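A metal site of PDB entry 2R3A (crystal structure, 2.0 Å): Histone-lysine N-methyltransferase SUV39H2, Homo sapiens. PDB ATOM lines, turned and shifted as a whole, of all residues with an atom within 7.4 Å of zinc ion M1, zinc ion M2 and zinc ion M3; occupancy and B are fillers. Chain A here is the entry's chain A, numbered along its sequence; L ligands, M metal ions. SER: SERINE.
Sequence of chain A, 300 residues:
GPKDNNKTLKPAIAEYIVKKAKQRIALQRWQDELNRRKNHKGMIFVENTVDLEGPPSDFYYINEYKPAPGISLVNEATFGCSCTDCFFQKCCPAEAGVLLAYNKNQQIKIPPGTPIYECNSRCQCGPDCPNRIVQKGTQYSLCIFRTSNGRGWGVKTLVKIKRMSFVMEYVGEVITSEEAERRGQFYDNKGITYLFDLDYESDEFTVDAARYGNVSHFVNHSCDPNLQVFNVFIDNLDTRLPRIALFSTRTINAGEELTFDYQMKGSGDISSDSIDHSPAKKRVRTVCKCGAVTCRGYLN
Zinc ion M3 is bound by the side-chain sulfur (SG) of Cys 125 (2.3 Å), the side-chain sulfur (SG) of Cys 119 (2.4 Å), the side-chain sulfur (SG) of Cys 86 (2.4 Å) and the side-chain sulfur (SG) of Cys 129 (2.4 Å).
Zinc ion M2 is bound by SG of Cys 86 (2.2 Å), SG of Cys 81 (2.4 Å), SG of Cys 83 (2.4 Å) and SG of Cys 91 (2.4 Å).
The nearest printed residue that does not touch zinc ion M1 is Asn 120 (4.5 Å).
The backbone NH (N) of Gly 126 lies within hydrogen-bond range of an oxygen (OXT) of the ligand (3.4 Å).
N of Cys 86 lies within hydrogen-bond range of OG of the ligand (2.7 Å).
Four residues have an atom within 4 Å of zinc ion M3: Cys 86, Cys 119, Cys 125 and Cys 129.
The side-chain sulfur (SG) of Cys 92 binds zinc ion M1 (2.3 Å).
SG of Cys 123 is bound to zinc ion M1 (2.4 Å).
Zinc ion M1 is bound by SG of Cys 81, at 2.4 Å.
SG of Cys 119 binds zinc ion M1 (2.4 Å).
Zinc ion M1 has four donor atoms within binding distance.
O of Asn 131 sits at hydrogen-bond distance from N of Cys 119 (3.1 Å).
N of Asn 120 lies close to SG of Cys 123, 3.2 Å away.
The backbone carbonyl oxygen of Lys 90 lies close to the side-chain sulfur of Cys 83 (3.4 Å).
The backbone carbonyl oxygen (O) of Cys 125 sits at hydrogen-bond distance from the guanidinium group (NH2) of Arg 132 (3.1 Å).
The backbone carbonyl oxygen (O) of Cys 81 is in hydrogen-bond range of the backbone NH (N) of Gln 124, 3.2 Å away.
The backbone NH (N) of Asn 131 lies close to the side-chain sulfur (SG) of Cys 129, 3.1 Å away.
Of the 28 residues printed, 5 come within 4 Å of zinc ion M2.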
ATOM      1  N   PHE A  79      -5.824 -10.165  -4.234  1.00  0.00           N
ATOM      2  CA  PHE A  79      -5.163  -9.645  -3.045  1.00  0.00           C
ATOM      3  C   PHE A  79      -6.206  -9.560  -1.916  1.00  0.00           C
ATOM      4  O   PHE A  79      -7.396  -9.259  -2.148  1.00  0.00           O
ATOM      5  CB  PHE A  79      -4.556  -8.248  -3.286  1.00  0.00           C
ATOM      6  CG  PHE A  79      -3.639  -8.158  -4.494  1.00  0.00           C
ATOM      7  CD1 PHE A  79      -2.324  -8.607  -4.422  1.00  0.00           C
ATOM      8  CD2 PHE A  79      -4.080  -7.568  -5.685  1.00  0.00           C
ATOM      9  CE1 PHE A  79      -1.464  -8.491  -5.525  1.00  0.00           C
ATOM     10  CE2 PHE A  79      -3.216  -7.454  -6.779  1.00  0.00           C
ATOM     11  CZ  PHE A  79      -1.908  -7.910  -6.693  1.00  0.00           C
ATOM     12  N   GLY A  80      -5.759  -9.844  -0.701  1.00  0.00           N
ATOM     13  CA  GLY A  80      -6.570  -9.622   0.465  1.00  0.00           C
ATOM     14  C   GLY A  80      -5.856  -8.662   1.384  1.00  0.00           C
ATOM     15  O   GLY A  80      -4.801  -8.119   1.047  1.00  0.00           O
ATOM     16  N   CYS A  81      -6.467  -8.476   2.554  1.00  0.00           N
ATOM     17  CA  CYS A  81      -5.918  -7.692   3.654  1.00  0.00           C
ATOM     18  C   CYS A  81      -4.977  -8.567   4.500  1.00  0.00           C
ATOM     19  O   CYS A  81      -4.949  -9.782   4.322  1.00  0.00           O
ATOM     20  CB  CYS A  81      -7.097  -7.217   4.527  1.00  0.00           C
ATOM     21  SG  CYS A  81      -7.941  -8.554   5.456  1.00  0.00           S
ATOM     22  N   SER A  82      -4.267  -7.951   5.455  1.00  0.00           N
ATOM     23  CA  SER A  82      -3.354  -8.665   6.362  1.00  0.00           C
ATOM     24  C   SER A  82      -3.615  -8.419   7.841  1.00  0.00           C
ATOM     25  O   SER A  82      -2.750  -8.804   8.689  1.00  0.00           O
ATOM     26  CB  SER A  82      -1.879  -8.313   6.091  1.00  0.00           C
ATOM     27  OG  SER A  82      -1.690  -7.738   4.830  1.00  0.00           O
ATOM     28  N   CYS A  83      -4.752  -7.773   8.147  1.00  0.00           N
ATOM     29  CA  CYS A  83      -5.240  -7.554   9.495  1.00  0.00           C
ATOM     30  C   CYS A  83      -5.144  -8.767  10.380  1.00  0.00           C
ATOM     31  O   CYS A  83      -5.422  -9.906   9.952  1.00  0.00           O
ATOM     32  CB  CYS A  83      -6.691  -7.056   9.490  1.00  0.00           C
ATOM     33  SG  CYS A  83      -7.103  -5.914   8.159  1.00  0.00           S
ATOM     34  N   THR A  84      -4.741  -8.505  11.620  1.00  0.00           N
ATOM     35  CA  THR A  84      -4.947  -9.444  12.713  1.00  0.00           C
ATOM     36  C   THR A  84      -6.284  -9.117  13.424  1.00  0.00           C
ATOM     37  O   THR A  84      -6.828  -9.944  14.152  1.00  0.00           O
ATOM     38  CB  THR A  84      -3.817  -9.399  13.732  1.00  0.00           C
ATOM     39  OG1 THR A  84      -3.547  -8.039  14.096  1.00  0.00           O
ATOM     40  CG2 THR A  84      -2.521 -10.061  13.186  1.00  0.00           C
ATOM     41  N   ASP A  85      -6.783  -7.907  13.199  1.00  0.00           N
ATOM     42  CA  ASP A  85      -8.097  -7.477  13.666  1.00  0.00           C
ATOM     43  C   ASP A  85      -8.778  -6.697  12.537  1.00  0.00           C
ATOM     44  O   ASP A  85      -8.613  -5.481  12.416  1.00  0.00           O
ATOM     45  CB  ASP A  85      -7.958  -6.608  14.918  1.00  0.00           C
ATOM     46  CG  ASP A  85      -9.293  -6.387  15.641  1.00  0.00           C
ATOM     47  OD1 ASP A  85     -10.361  -6.655  15.081  1.00  0.00           O
ATOM     48  OD2 ASP A  85      -9.241  -5.928  16.807  1.00  0.00           O
ATOM     49  N   CYS A  86      -9.515  -7.413  11.674  1.00  0.00           N
ATOM     50  CA  CYS A  86     -10.187  -6.765  10.517  1.00  0.00           C
ATOM     51  C   CYS A  86     -11.260  -5.774  10.935  1.00  0.00           C
ATOM     52  O   CYS A  86     -11.602  -4.862  10.181  1.00  0.00           O
ATOM     53  CB  CYS A  86     -10.814  -7.806   9.618  1.00  0.00           C
ATOM     54  SG  CYS A  86      -9.608  -8.725   8.704  1.00  0.00           S
ATOM     55  N   PHE A  87     -11.803  -5.948  12.130  1.00  0.00           N
ATOM     56  CA  PHE A  87     -12.806  -5.007  12.633  1.00  0.00           C
ATOM     57  C   PHE A  87     -12.240  -3.575  12.877  1.00  0.00           C
ATOM     58  O   PHE A  87     -12.936  -2.572  12.670  1.00  0.00           O
ATOM     59  CB  PHE A  87     -13.512  -5.567  13.879  1.00  0.00           C
ATOM     60  CG  PHE A  87     -14.756  -4.807  14.244  1.00  0.00           C
ATOM     61  CD1 PHE A  87     -15.955  -5.030  13.549  1.00  0.00           C
ATOM     62  CD2 PHE A  87     -14.734  -3.820  15.240  1.00  0.00           C
ATOM     63  CE1 PHE A  87     -17.111  -4.282  13.862  1.00  0.00           C
ATOM     64  CE2 PHE A  87     -15.889  -3.083  15.562  1.00  0.00           C
ATOM     65  CZ  PHE A  87     -17.080  -3.309  14.863  1.00  0.00           C
ATOM     66  N   GLN A  89      -8.602  -2.590  12.066  1.00  0.00           N
ATOM     67  CA  GLN A  89      -7.481  -2.199  11.188  1.00  0.00           C
ATOM     68  C   GLN A  89      -7.977  -1.804   9.795  1.00  0.00           C
ATOM     69  O   GLN A  89      -9.162  -1.964   9.486  1.00  0.00           O
ATOM     70  CB  GLN A  89      -6.432  -3.327  11.133  1.00  0.00           C
ATOM     71  CG  GLN A  89      -5.798  -3.590  12.496  1.00  0.00           C
ATOM     72  CD  GLN A  89      -4.736  -4.638  12.432  1.00  0.00           C
ATOM     73  OE1 GLN A  89      -4.912  -5.687  11.811  1.00  0.00           O
ATOM     74  NE2 GLN A  89      -3.586  -4.369  13.109  1.00  0.00           N
ATOM     75  N   LYS A  90      -7.087  -1.280   8.969  1.00  0.00           N
ATOM     76  CA  LYS A  90      -7.466  -0.903   7.587  1.00  0.00           C
ATOM     77  C   LYS A  90      -7.566  -2.180   6.766  1.00  0.00           C
ATOM     78  O   LYS A  90      -6.581  -2.902   6.612  1.00  0.00           O
ATOM     79  CB  LYS A  90      -6.441   0.044   6.958  1.00  0.00           C
ATOM     80  CG  LYS A  90      -6.641   1.505   7.271  1.00  0.00           C
ATOM     81  CD  LYS A  90      -5.486   2.340   6.727  1.00  0.00           C
ATOM     82  CE  LYS A  90      -4.621   2.914   7.861  1.00  0.00           C
ATOM     83  NZ  LYS A  90      -5.267   4.149   8.391  1.00  0.00           N
ATOM     84  N   CYS A  91      -8.755  -2.467   6.260  1.00  0.00           N
ATOM     85  CA  CYS A  91      -9.119  -3.781   5.790  1.00  0.00           C
ATOM     86  C   CYS A  91      -9.667  -3.690   4.349  1.00  0.00           C
ATOM     87  O   CYS A  91      -9.554  -2.649   3.707  1.00  0.00           O
ATOM     88  CB  CYS A  91     -10.149  -4.344   6.765  1.00  0.00           C
ATOM     89  SG  CYS A  91     -10.806  -5.973   6.434  1.00  0.00           S
ATOM     90  N   CYS A  92     -10.232  -4.789   3.858  1.00  0.00           N
ATOM     91  CA  CYS A  92     -10.753  -4.808   2.484  1.00  0.00           C
ATOM     92  C   CYS A  92     -11.707  -3.677   2.086  1.00  0.00           C
ATOM     93  O   CYS A  92     -11.541  -3.084   1.003  1.00  0.00           O
ATOM     94  CB  CYS A  92     -11.344  -6.184   2.145  1.00  0.00           C
ATOM     95  SG  CYS A  92     -10.114  -7.579   2.182  1.00  0.00           S
ATOM     96  N   PRO A  93     -12.726  -3.375   2.936  1.00  0.00           N
ATOM     97  CA  PRO A  93     -13.577  -2.249   2.513  1.00  0.00           C
ATOM     98  C   PRO A  93     -12.803  -0.923   2.354  1.00  0.00           C
ATOM     99  O   PRO A  93     -13.002  -0.211   1.372  1.00  0.00           O
ATOM    100  CB  PRO A  93     -14.649  -2.133   3.635  1.00  0.00           C
ATOM    101  CG  PRO A  93     -14.521  -3.339   4.461  1.00  0.00           C
ATOM    102  CD  PRO A  93     -13.147  -3.921   4.229  1.00  0.00           C
ATOM    103  N   TYR A 117     -17.823  -5.251   0.671  1.00  0.00           N
ATOM    104  CA  TYR A 117     -16.551  -5.883   0.294  1.00  0.00           C
ATOM    105  C   TYR A 117     -16.148  -6.713   1.491  1.00  0.00           C
ATOM    106  O   TYR A 117     -15.681  -6.181   2.517  1.00  0.00           O
ATOM    107  CB  TYR A 117     -15.453  -4.849  -0.063  1.00  0.00           C
ATOM    108  CG  TYR A 117     -15.623  -4.257  -1.444  1.00  0.00           C
ATOM    109  CD1 TYR A 117     -14.953  -4.807  -2.553  1.00  0.00           C
ATOM    110  CD2 TYR A 117     -16.447  -3.157  -1.650  1.00  0.00           C
ATOM    111  CE1 TYR A 117     -15.132  -4.288  -3.804  1.00  0.00           C
ATOM    112  CE2 TYR A 117     -16.645  -2.623  -2.925  1.00  0.00           C
ATOM    113  CZ  TYR A 117     -15.972  -3.193  -3.992  1.00  0.00           C
ATOM    114  OH  TYR A 117     -16.107  -2.670  -5.275  1.00  0.00           O
ATOM    115  N   GLU A 118     -16.387  -8.013   1.406  1.00  0.00           N
ATOM    116  CA  GLU A 118     -16.033  -8.928   2.497  1.00  0.00           C
ATOM    117  C   GLU A 118     -14.585  -9.396   2.307  1.00  0.00           C
ATOM    118  O   GLU A 118     -14.016  -9.278   1.206  1.00  0.00           O
ATOM    119  CB  GLU A 118     -16.933 -10.177   2.533  1.00  0.00           C
ATOM    120  CG  GLU A 118     -18.429  -9.861   2.742  1.00  0.00           C
ATOM    121  CD  GLU A 118     -19.189 -11.002   3.386  1.00  0.00           C
ATOM    122  OE1 GLU A 118     -18.783 -12.179   3.302  1.00  0.00           O
ATOM    123  OE2 GLU A 118     -20.241 -10.734   4.004  1.00  0.00           O
ATOM    124  N   CYS A 119     -13.994  -9.961   3.354  1.00  0.00           N
ATOM    125  CA  CYS A 119     -12.700 -10.574   3.222  1.00  0.00           C
ATOM    126  C   CYS A 119     -12.852 -11.865   2.402  1.00  0.00           C
ATOM    127  O   CYS A 119     -13.959 -12.420   2.287  1.00  0.00           O
ATOM    128  CB  CYS A 119     -12.107 -10.875   4.601  1.00  0.00           C
ATOM    129  SG  CYS A 119     -11.685  -9.405   5.501  1.00  0.00           S
ATOM    130  N   ASN A 120     -11.744 -12.328   1.828  1.00  0.00           N
ATOM    131  CA  ASN A 120     -11.812 -13.335   0.775  1.00  0.00           C
ATOM    132  C   ASN A 120     -10.725 -14.395   0.985  1.00  0.00           C
ATOM    133  O   ASN A 120     -10.079 -14.396   2.057  1.00  0.00           O
ATOM    134  CB  ASN A 120     -11.748 -12.663  -0.597  1.00  0.00           C
ATOM    135  CG  ASN A 120     -10.446 -11.879  -0.827  1.00  0.00           C
ATOM    136  OD1 ASN A 120      -9.353 -12.449  -0.851  1.00  0.00           O
ATOM    137  ND2 ASN A 120     -10.563 -10.583  -1.009  1.00  0.00           N
ATOM    138  N   ARG A 122      -7.913 -14.782  -0.167  1.00  0.00           N
ATOM    139  CA  ARG A 122      -6.577 -14.225  -0.136  1.00  0.00           C
ATOM    140  C   ARG A 122      -6.255 -13.459   1.133  1.00  0.00           C
ATOM    141  O   ARG A 122      -5.101 -13.146   1.360  1.00  0.00           O
ATOM    142  CB  ARG A 122      -6.332 -13.341  -1.372  1.00  0.00           C
ATOM    143  N   CYS A 123      -7.254 -13.111   1.967  1.00  0.00           N
ATOM    144  CA  CYS A 123      -6.972 -12.406   3.226  1.00  0.00           C
ATOM    145  C   CYS A 123      -6.343 -13.367   4.242  1.00  0.00           C
ATOM    146  O   CYS A 123      -6.587 -14.579   4.178  1.00  0.00           O
ATOM    147  CB  CYS A 123      -8.260 -11.829   3.827  1.00  0.00           C
ATOM    148  SG  CYS A 123      -9.113 -10.716   2.696  1.00  0.00           S
ATOM    149  N   GLN A 124      -5.590 -12.819   5.193  1.00  0.00           N
ATOM    150  CA  GLN A 124      -4.936 -13.617   6.233  1.00  0.00           C
ATOM    151  C   GLN A 124      -5.879 -14.151   7.292  1.00  0.00           C
ATOM    152  O   GLN A 124      -5.568 -15.164   7.964  1.00  0.00           O
ATOM    153  CB  GLN A 124      -3.829 -12.824   6.933  1.00  0.00           C
ATOM    154  CG  GLN A 124      -2.556 -12.482   6.092  1.00  0.00           C
ATOM    155  CD  GLN A 124      -1.857 -13.716   5.526  1.00  0.00           C
ATOM    156  OE1 GLN A 124      -1.414 -14.620   6.267  1.00  0.00           O
ATOM    157  NE2 GLN A 124      -1.751 -13.772   4.213  1.00  0.00           N
ATOM    158  N   CYS A 125      -7.015 -13.440   7.482  1.00  0.00           N
ATOM    159  CA  CYS A 125      -7.972 -13.736   8.547  1.00  0.00           C
ATOM    160  C   CYS A 125      -8.706 -15.047   8.324  1.00  0.00           C
ATOM    161  O   CYS A 125      -8.911 -15.484   7.187  1.00  0.00           O
ATOM    162  CB  CYS A 125      -8.993 -12.602   8.678  1.00  0.00           C
ATOM    163  SG  CYS A 125      -9.899 -12.282   7.103  1.00  0.00           S
ATOM    164  N   GLY A 126      -9.125 -15.649   9.424  1.00  0.00           N
ATOM    165  CA  GLY A 126      -9.869 -16.901   9.399  1.00  0.00           C
ATOM    166  C   GLY A 126     -11.381 -16.662   9.321  1.00  0.00           C
ATOM    167  O   GLY A 126     -11.836 -15.523   9.191  1.00  0.00           O
ATOM    168  N   ASP A 128     -13.897 -16.633  11.387  1.00  0.00           N
ATOM    169  CA  ASP A 128     -14.632 -15.838  12.349  1.00  0.00           C
ATOM    170  C   ASP A 128     -14.290 -14.340  12.283  1.00  0.00           C
ATOM    171  O   ASP A 128     -14.659 -13.556  13.164  1.00  0.00           O
ATOM    172  CB  ASP A 128     -14.550 -16.494  13.743  1.00  0.00           C
ATOM    173  CG  ASP A 128     -15.050 -17.985  13.750  1.00  0.00           C
ATOM    174  OD1 ASP A 128     -15.992 -18.363  12.978  1.00  0.00           O
ATOM    175  OD2 ASP A 128     -14.493 -18.787  14.548  1.00  0.00           O
ATOM    176  N   CYS A 129     -13.639 -13.921  11.193  1.00  0.00           N
ATOM    177  CA  CYS A 129     -13.538 -12.508  10.844  1.00  0.00           C
ATOM    178  C   CYS A 129     -14.952 -11.847  10.770  1.00  0.00           C
ATOM    179  O   CYS A 129     -15.877 -12.360  10.111  1.00  0.00           O
ATOM    180  CB  CYS A 129     -12.808 -12.321   9.520  1.00  0.00           C
ATOM    181  SG  CYS A 129     -12.873 -10.627   8.885  1.00  0.00           S
ATOM    182  N   PRO A 130     -15.118 -10.700  11.458  1.00  0.00           N
ATOM    183  CA  PRO A 130     -16.416 -10.050  11.485  1.00  0.00           C
ATOM    184  C   PRO A 130     -16.768  -9.524  10.093  1.00  0.00           C
ATOM    185  O   PRO A 130     -17.876  -9.048   9.895  1.00  0.00           O
ATOM    186  CB  PRO A 130     -16.199  -8.877  12.452  1.00  0.00           C
ATOM    187  CG  PRO A 130     -14.738  -8.584  12.314  1.00  0.00           C
ATOM    188  CD  PRO A 130     -14.119  -9.929  12.239  1.00  0.00           C
ATOM    189  N   ASN A 131     -15.799  -9.562   9.157  1.00  0.00           N
ATOM    190  CA  ASN A 131     -16.077  -9.168   7.753  1.00  0.00           C
ATOM    191  C   ASN A 131     -16.332 -10.368   6.822  1.00  0.00           C
ATOM    192  O   ASN A 131     -16.161 -10.292   5.613  1.00  0.00           O
ATOM    193  CB  ASN A 131     -15.038  -8.154   7.245  1.00  0.00           C
ATOM    194  CG  ASN A 131     -15.415  -7.501   5.898  1.00  0.00           C
ATOM    195  OD1 ASN A 131     -14.519  -7.123   5.123  1.00  0.00           O
ATOM    196  ND2 ASN A 131     -16.691  -7.320   5.651  1.00  0.00           N
ATOM    197  N   ARG A 132     -16.782 -11.480   7.382  1.00  0.00           N
ATOM    198  CA  ARG A 132     -17.130 -12.653   6.552  1.00  0.00           C
ATOM    199  C   ARG A 132     -18.520 -13.131   6.972  1.00  0.00           C
ATOM    200  O   ARG A 132     -18.641 -13.974   7.857  1.00  0.00           O
ATOM    201  CB  ARG A 132     -16.095 -13.770   6.770  1.00  0.00           C
ATOM    202  CG  ARG A 132     -14.659 -13.473   6.247  1.00  0.00           C
ATOM    203  CD  ARG A 132     -13.704 -14.611   6.699  1.00  0.00           C
ATOM    204  NE  ARG A 132     -12.311 -14.464   6.248  1.00  0.00           N
ATOM    205  CZ  ARG A 132     -11.863 -14.746   5.033  1.00  0.00           C
ATOM    206  NH1 ARG A 132     -12.684 -15.186   4.079  1.00  0.00           N
ATOM    207  NH2 ARG A 132     -10.572 -14.606   4.761  1.00  0.00           N
HETATM  208  N   SER L   1     -11.310 -11.815  14.200  1.00  0.00           N
HETATM  209  CA  SER L   1     -10.656 -12.235  12.911  1.00  0.00           C
HETATM  210  C   SER L   1     -10.007 -13.637  12.917  1.00  0.00           C
HETATM  211  O   SER L   1     -10.572 -14.593  13.509  1.00  0.00           O
HETATM  212  CB  SER L   1      -9.696 -11.131  12.415  1.00  0.00           C
HETATM  213  OG  SER L   1     -10.382  -9.890  12.335  1.00  0.00           O
HETATM  214  OXT SER L   1      -8.929 -13.870  12.300  1.00  0.00           O
HETATM  215 ZN    ZN M   1      -9.829  -8.900   4.007  1.00  0.00          ZN
HETATM  216 ZN    ZN M   2      -8.874  -7.218   7.210  1.00  0.00          ZN
HETATM  217 ZN    ZN M   3     -10.925 -10.302   7.544  1.00  0.00          ZN
